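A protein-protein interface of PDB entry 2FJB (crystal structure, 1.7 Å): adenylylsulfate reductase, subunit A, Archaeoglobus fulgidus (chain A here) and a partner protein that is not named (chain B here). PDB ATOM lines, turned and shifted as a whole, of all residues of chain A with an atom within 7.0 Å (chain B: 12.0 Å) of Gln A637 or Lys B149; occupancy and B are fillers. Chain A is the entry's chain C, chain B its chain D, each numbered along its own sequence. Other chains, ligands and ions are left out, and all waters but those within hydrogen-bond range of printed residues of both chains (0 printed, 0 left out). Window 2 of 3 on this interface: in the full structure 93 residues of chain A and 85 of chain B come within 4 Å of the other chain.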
ATOM      1  N   VAL A  93      27.257  11.933 -24.363  1.00  0.00           N
ATOM      2  CA  VAL A  93      25.945  12.008 -24.996  1.00  0.00           C
ATOM      3  C   VAL A  93      26.089  11.997 -26.515  1.00  0.00           C
ATOM      4  O   VAL A  93      25.355  11.291 -27.209  1.00  0.00           O
ATOM      5  CB  VAL A  93      25.174  13.269 -24.542  1.00  0.00           C
ATOM      6  CG1 VAL A  93      23.870  13.398 -25.321  1.00  0.00           C
ATOM      7  CG2 VAL A  93      24.869  13.176 -23.051  1.00  0.00           C
ATOM      8  N   THR A  97      24.507   9.167 -29.144  1.00  0.00           N
ATOM      9  CA  THR A  97      23.585   9.535 -30.220  1.00  0.00           C
ATOM     10  C   THR A  97      24.132   9.155 -31.593  1.00  0.00           C
ATOM     11  O   THR A  97      23.401   8.639 -32.440  1.00  0.00           O
ATOM     12  CB  THR A  97      23.272  11.051 -30.201  1.00  0.00           C
ATOM     13  OG1 THR A  97      22.506  11.356 -29.031  1.00  0.00           O
ATOM     14  CG2 THR A  97      22.470  11.457 -31.436  1.00  0.00           C
ATOM     15  N   ALA A 104      18.577   8.941 -30.149  1.00  0.00           N
ATOM     16  CA  ALA A 104      18.684   8.567 -28.745  1.00  0.00           C
ATOM     17  C   ALA A 104      18.007   9.637 -27.899  1.00  0.00           C
ATOM     18  O   ALA A 104      18.057  10.821 -28.239  1.00  0.00           O
ATOM     19  CB  ALA A 104      20.144   8.431 -28.345  1.00  0.00           C
ATOM     20  N   GLU A 106      18.375  11.881 -25.518  1.00  0.00           N
ATOM     21  CA  GLU A 106      19.505  12.484 -24.831  1.00  0.00           C
ATOM     22  C   GLU A 106      19.230  12.912 -23.398  1.00  0.00           C
ATOM     23  O   GLU A 106      20.153  12.986 -22.590  1.00  0.00           O
ATOM     24  CB  GLU A 106      20.048  13.653 -25.662  1.00  0.00           C
ATOM     25  CG  GLU A 106      20.422  13.219 -27.073  1.00  0.00           C
ATOM     26  CD  GLU A 106      21.205  14.268 -27.825  1.00  0.00           C
ATOM     27  OE1 GLU A 106      21.136  15.450 -27.424  1.00  0.00           O
ATOM     28  OE2 GLU A 106      21.873  13.913 -28.822  1.00  0.00           O
ATOM     29  N   PRO A 414      12.770  17.599 -22.637  1.00  0.00           N
ATOM     30  CA  PRO A 414      12.092  18.692 -23.337  1.00  0.00           C
ATOM     31  C   PRO A 414      10.597  18.400 -23.468  1.00  0.00           C
ATOM     32  O   PRO A 414      10.176  17.246 -23.410  1.00  0.00           O
ATOM     33  CB  PRO A 414      12.799  18.720 -24.685  1.00  0.00           C
ATOM     34  CG  PRO A 414      13.082  17.268 -24.926  1.00  0.00           C
ATOM     35  CD  PRO A 414      13.589  16.805 -23.574  1.00  0.00           C
ATOM     36  N   TYR A 417       9.201  15.563 -25.599  1.00  0.00           N
ATOM     37  CA  TYR A 417       9.205  14.180 -25.114  1.00  0.00           C
ATOM     38  C   TYR A 417       8.279  13.883 -23.935  1.00  0.00           C
ATOM     39  O   TYR A 417       8.194  12.739 -23.493  1.00  0.00           O
ATOM     40  CB  TYR A 417      10.629  13.784 -24.703  1.00  0.00           C
ATOM     41  CG  TYR A 417      11.658  13.772 -25.815  1.00  0.00           C
ATOM     42  CD1 TYR A 417      13.024  13.808 -25.517  1.00  0.00           C
ATOM     43  CD2 TYR A 417      11.281  13.695 -27.157  1.00  0.00           C
ATOM     44  CE1 TYR A 417      13.986  13.766 -26.522  1.00  0.00           C
ATOM     45  CE2 TYR A 417      12.238  13.652 -28.173  1.00  0.00           C
ATOM     46  CZ  TYR A 417      13.590  13.688 -27.845  1.00  0.00           C
ATOM     47  OH  TYR A 417      14.547  13.647 -28.831  1.00  0.00           O
ATOM     48  N   LYS A 614      13.828  10.676 -38.878  1.00  0.00           N
ATOM     49  CA  LYS A 614      14.730  10.960 -37.766  1.00  0.00           C
ATOM     50  C   LYS A 614      13.810  11.179 -36.577  1.00  0.00           C
ATOM     51  O   LYS A 614      13.701  12.278 -36.027  1.00  0.00           O
ATOM     52  CB  LYS A 614      15.569  12.210 -38.035  1.00  0.00           C
ATOM     53  CG  LYS A 614      16.749  12.310 -37.087  1.00  0.00           C
ATOM     54  CD  LYS A 614      17.645  13.498 -37.382  1.00  0.00           C
ATOM     55  CE  LYS A 614      18.869  13.458 -36.477  1.00  0.00           C
ATOM     56  NZ  LYS A 614      19.759  14.638 -36.663  1.00  0.00           N
ATOM     57  N   TYR A 635      13.057  13.377 -33.161  1.00  0.00           N
ATOM     58  CA  TYR A 635      14.209  13.499 -32.287  1.00  0.00           C
ATOM     59  C   TYR A 635      14.562  14.979 -32.224  1.00  0.00           C
ATOM     60  O   TYR A 635      14.425  15.701 -33.213  1.00  0.00           O
ATOM     61  CB  TYR A 635      15.406  12.733 -32.871  1.00  0.00           C
ATOM     62  CG  TYR A 635      16.767  13.229 -32.396  1.00  0.00           C
ATOM     63  CD1 TYR A 635      17.382  12.689 -31.265  1.00  0.00           C
ATOM     64  CD2 TYR A 635      17.430  14.252 -33.078  1.00  0.00           C
ATOM     65  CE1 TYR A 635      18.630  13.155 -30.826  1.00  0.00           C
ATOM     66  CE2 TYR A 635      18.670  14.730 -32.645  1.00  0.00           C
ATOM     67  CZ  TYR A 635      19.265  14.179 -31.523  1.00  0.00           C
ATOM     68  OH  TYR A 635      20.486  14.658 -31.106  1.00  0.00           O
ATOM     69  N   VAL A 636      14.980  15.428 -31.049  1.00  0.00           N
ATOM     70  CA  VAL A 636      15.433  16.801 -30.872  1.00  0.00           C
ATOM     71  C   VAL A 636      16.716  16.677 -30.067  1.00  0.00           C
ATOM     72  O   VAL A 636      16.807  15.837 -29.165  1.00  0.00           O
ATOM     73  CB  VAL A 636      14.421  17.688 -30.095  1.00  0.00           C
ATOM     74  CG1 VAL A 636      13.201  17.953 -30.955  1.00  0.00           C
ATOM     75  CG2 VAL A 636      14.031  17.030 -28.786  1.00  0.00           C
ATOM     76  N   GLN A 637      17.719  17.477 -30.411  1.00  0.00           N
ATOM     77  CA  GLN A 637      18.980  17.431 -29.686  1.00  0.00           C
ATOM     78  C   GLN A 637      18.778  18.192 -28.383  1.00  0.00           C
ATOM     79  O   GLN A 637      18.438  19.373 -28.393  1.00  0.00           O
ATOM     80  CB  GLN A 637      20.105  18.068 -30.503  1.00  0.00           C
ATOM     81  CG  GLN A 637      21.481  17.816 -29.900  1.00  0.00           C
ATOM     82  CD  GLN A 637      22.609  18.382 -30.737  1.00  0.00           C
ATOM     83  OE1 GLN A 637      22.551  18.369 -31.966  1.00  0.00           O
ATOM     84  NE2 GLN A 637      23.654  18.860 -30.074  1.00  0.00           N
ATOM     85  N   VAL A 638      18.984  17.504 -27.265  1.00  0.00           N
ATOM     86  CA  VAL A 638      18.798  18.093 -25.945  1.00  0.00           C
ATOM     87  C   VAL A 638      20.080  18.654 -25.343  1.00  0.00           C
ATOM     88  O   VAL A 638      20.073  19.710 -24.707  1.00  0.00           O
ATOM     89  CB  VAL A 638      18.210  17.041 -24.973  1.00  0.00           C
ATOM     90  CG1 VAL A 638      18.077  17.627 -23.575  1.00  0.00           C
ATOM     91  CG2 VAL A 638      16.859  16.563 -25.490  1.00  0.00           C
ATOM     92  N   ILE A 639      21.181  17.941 -25.551  1.00  0.00           N
ATOM     93  CA  ILE A 639      22.471  18.338 -25.006  1.00  0.00           C
ATOM     94  C   ILE A 639      23.346  19.031 -26.043  1.00  0.00           C
ATOM     95  O   ILE A 639      23.308  18.704 -27.229  1.00  0.00           O
ATOM     96  CB  ILE A 639      23.216  17.103 -24.441  1.00  0.00           C
ATOM     97  CG1 ILE A 639      22.383  16.467 -23.326  1.00  0.00           C
ATOM     98  CG2 ILE A 639      24.595  17.497 -23.927  1.00  0.00           C
ATOM     99  CD1 ILE A 639      22.069  17.404 -22.164  1.00  0.00           C
ATOM    100  N   GLU A 640      24.128  20.000 -25.581  1.00  0.00           N
ATOM    101  CA  GLU A 640      25.018  20.746 -26.452  1.00  0.00           C
ATOM    102  C   GLU A 640      26.239  19.939 -26.886  1.00  0.00           C
ATOM    103  O   GLU A 640      27.026  19.480 -26.057  1.00  0.00           O
ATOM    104  CB  GLU A 640      25.480  22.029 -25.759  1.00  0.00           C
ATOM    105  CG  GLU A 640      26.519  22.811 -26.548  1.00  0.00           C
ATOM    106  CD  GLU A 640      26.946  24.085 -25.850  1.00  0.00           C
ATOM    107  OE1 GLU A 640      26.091  24.978 -25.663  1.00  0.00           O
ATOM    108  OE2 GLU A 640      28.136  24.192 -25.489  1.00  0.00           O
ATOM    109  N   TRP A 641      26.371  19.773 -28.199  1.00  0.00           N
ATOM    110  CA  TRP A 641      27.488  19.066 -28.817  1.00  0.00           C
ATOM    111  C   TRP A 641      27.379  19.225 -30.325  1.00  0.00           C
ATOM    112  O   TRP A 641      26.297  19.487 -30.857  1.00  0.00           O
ATOM    113  CB  TRP A 641      27.495  17.568 -28.458  1.00  0.00           C
ATOM    114  CG  TRP A 641      26.299  16.766 -28.926  1.00  0.00           C
ATOM    115  CD1 TRP A 641      25.206  16.415 -28.181  1.00  0.00           C
ATOM    116  CD2 TRP A 641      26.094  16.192 -30.228  1.00  0.00           C
ATOM    117  NE1 TRP A 641      24.340  15.658 -28.933  1.00  0.00           N
ATOM    118  CE2 TRP A 641      24.857  15.508 -30.192  1.00  0.00           C
ATOM    119  CE3 TRP A 641      26.833  16.190 -31.419  1.00  0.00           C
ATOM    120  CZ2 TRP A 641      24.343  14.826 -31.303  1.00  0.00           C
ATOM    121  CZ3 TRP A 641      26.322  15.510 -32.525  1.00  0.00           C
ATOM    122  CH2 TRP A 641      25.087  14.839 -32.456  1.00  0.00           C
ATOM    123  N   SER A 642      28.505  19.090 -31.013  1.00  0.00           N
ATOM    124  CA  SER A 642      28.522  19.200 -32.463  1.00  0.00           C
ATOM    125  C   SER A 642      29.421  18.102 -33.007  1.00  0.00           C
ATOM    126  O   SER A 642      30.288  17.589 -32.300  1.00  0.00           O
ATOM    127  CB  SER A 642      29.037  20.578 -32.895  1.00  0.00           C
ATOM    128  OG  SER A 642      30.347  20.813 -32.412  1.00  0.00           O
ATOM    129  N   GLN B 145      27.145  18.915 -13.874  1.00  0.00           N
ATOM    130  CA  GLN B 145      26.286  19.689 -14.756  1.00  0.00           C
ATOM    131  C   GLN B 145      26.550  19.257 -16.192  1.00  0.00           C
ATOM    132  O   GLN B 145      27.661  18.848 -16.531  1.00  0.00           O
ATOM    133  CB  GLN B 145      26.581  21.185 -14.611  1.00  0.00           C
ATOM    134  CG  GLN B 145      26.277  21.748 -13.233  1.00  0.00           C
ATOM    135  CD  GLN B 145      24.797  21.732 -12.915  1.00  0.00           C
ATOM    136  OE1 GLN B 145      24.000  22.374 -13.599  1.00  0.00           O
ATOM    137  NE2 GLN B 145      24.420  20.994 -11.876  1.00  0.00           N
ATOM    138  N   VAL B 146      25.518  19.329 -17.024  1.00  0.00           N
ATOM    139  CA  VAL B 146      25.648  18.982 -18.432  1.00  0.00           C
ATOM    140  C   VAL B 146      25.000  20.117 -19.216  1.00  0.00           C
ATOM    141  O   VAL B 146      23.877  20.532 -18.917  1.00  0.00           O
ATOM    142  CB  VAL B 146      24.959  17.633 -18.761  1.00  0.00           C
ATOM    143  CG1 VAL B 146      23.467  17.722 -18.485  1.00  0.00           C
ATOM    144  CG2 VAL B 146      25.226  17.255 -20.217  1.00  0.00           C
ATOM    145  N   LYS B 147      25.725  20.631 -20.203  1.00  0.00           N
ATOM    146  CA  LYS B 147      25.245  21.739 -21.021  1.00  0.00           C
ATOM    147  C   LYS B 147      24.082  21.374 -21.933  1.00  0.00           C
ATOM    148  O   LYS B 147      24.208  20.517 -22.807  1.00  0.00           O
ATOM    149  CB  LYS B 147      26.392  22.292 -21.871  1.00  0.00           C
ATOM    150  CG  LYS B 147      27.628  22.695 -21.077  1.00  0.00           C
ATOM    151  CD  LYS B 147      28.714  23.242 -21.993  1.00  0.00           C
ATOM    152  CE  LYS B 147      29.955  23.648 -21.211  1.00  0.00           C
ATOM    153  NZ  LYS B 147      30.569  22.488 -20.503  1.00  0.00           N
ATOM    154  N   LYS B 148      22.947  22.031 -21.730  1.00  0.00           N
ATOM    155  CA  LYS B 148      21.782  21.782 -22.565  1.00  0.00           C
ATOM    156  C   LYS B 148      21.946  22.613 -23.826  1.00  0.00           C
ATOM    157  O   LYS B 148      22.505  23.713 -23.787  1.00  0.00           O
ATOM    158  CB  LYS B 148      20.498  22.168 -21.830  1.00  0.00           C
ATOM    159  CG  LYS B 148      20.215  21.295 -20.617  1.00  0.00           C
ATOM    160  CD  LYS B 148      18.918  21.685 -19.915  1.00  0.00           C
ATOM    161  CE  LYS B 148      17.706  21.381 -20.777  1.00  0.00           C
ATOM    162  NZ  LYS B 148      16.427  21.643 -20.056  1.00  0.00           N
ATOM    163  N   LYS B 149      21.471  22.090 -24.948  1.00  0.00           N
ATOM    164  CA  LYS B 149      21.607  22.809 -26.203  1.00  0.00           C
ATOM    165  C   LYS B 149      20.735  24.056 -26.224  1.00  0.00           C
ATOM    166  O   LYS B 149      19.553  24.005 -25.892  1.00  0.00           O
ATOM    167  CB  LYS B 149      21.237  21.917 -27.385  1.00  0.00           C
ATOM    168  CG  LYS B 149      21.781  22.461 -28.689  1.00  0.00           C
ATOM    169  CD  LYS B 149      21.044  21.933 -29.897  1.00  0.00           C
ATOM    170  CE  LYS B 149      21.556  22.625 -31.151  1.00  0.00           C
ATOM    171  NZ  LYS B 149      20.612  22.479 -32.287  1.00  0.00           N
ATOM    172  N   ALA B 150      21.328  25.177 -26.620  1.00  0.00           N
ATOM    173  CA  ALA B 150      20.613  26.447 -26.692  1.00  0.00           C
ATOM    174  C   ALA B 150      19.477  26.377 -27.709  1.00  0.00           C
ATOM    175  O   ALA B 150      19.651  26.916 -28.821  1.00  0.00           O
ATOM    176  CB  ALA B 150      21.578  27.568 -27.060  1.00  0.00           C
ATOM    177  OXT ALA B 150      18.432  25.771 -27.388  1.00  0.00           O
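OE1 of Glu A106 sits at hydrogen-bond distance from N of Val A638, 3.0 Å away.
N of Ile A639 is in hydrogen-bond range of OE1 of Glu A106.
O of Ile A639 sits at hydrogen-bond distance from NE2 of Gln A637 (2.9 Å).
NE2 of Gln A637 sits at hydrogen-bond distance from O of Trp A641 (2.8 Å).
Lys B149 touches Gln A637 (CB to O, 3.9 Å).
Lys B148 touches Val A638 (CA to O, 3.4 Å).
Ile A639 touches Val B146.
CG2 of Ile A639 touches O of Lys B147 (3.2 Å).
Lys B149 touches Ile A639.
Glu A640 touches Lys B148 (N to C, 3.8 Å).
Among the printed residues, 9 pairs touch across the chains.
Val A93 touches none of the printed residues of chain B.
No residue of chain B comes within 4 Å of Glu A106.
No residue of chain B comes within 4 Å of Tyr A635.
No residue of chain B comes within 4 Å of Val A636.
Of chain B, only Lys B149 (3.9 Å) comes within 4 Å of Gln A637.
Glu A640 touches just these residues of chain B: Lys B147, Lys B148 and Lys B149.
Printed residues of chain A within 4 Å of Val B146: Ile A639.
Of the printed residues of chain A, Lys B147 touches Ile A639 (3.2 Å) and Glu A640 (2.8 Å).
Of the printed residues of chain A, Lys B148 touches Val A638 (3.4 Å) and Glu A640 (3.8 Å).
Lys B149 touches four residues of chain A.
The nearest residue of chain A that does not touch Lys B149 is Trp A641 (5.3 Å).
The nearest printed residue of chain A that does not touch Val B146 is Val A93 (5.0 Å).
The backbone carbonyl oxygen of Val A638 sits at hydrogen-bond distance from the backbone NH of Lys B149 (2.8 Å).
N of Glu A640 sits at hydrogen-bond distance from O of Lys B147 (2.8 Å).
The backbone NH (N) of Lys B149 sits close to the backbone NH (N) of Glu A640.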
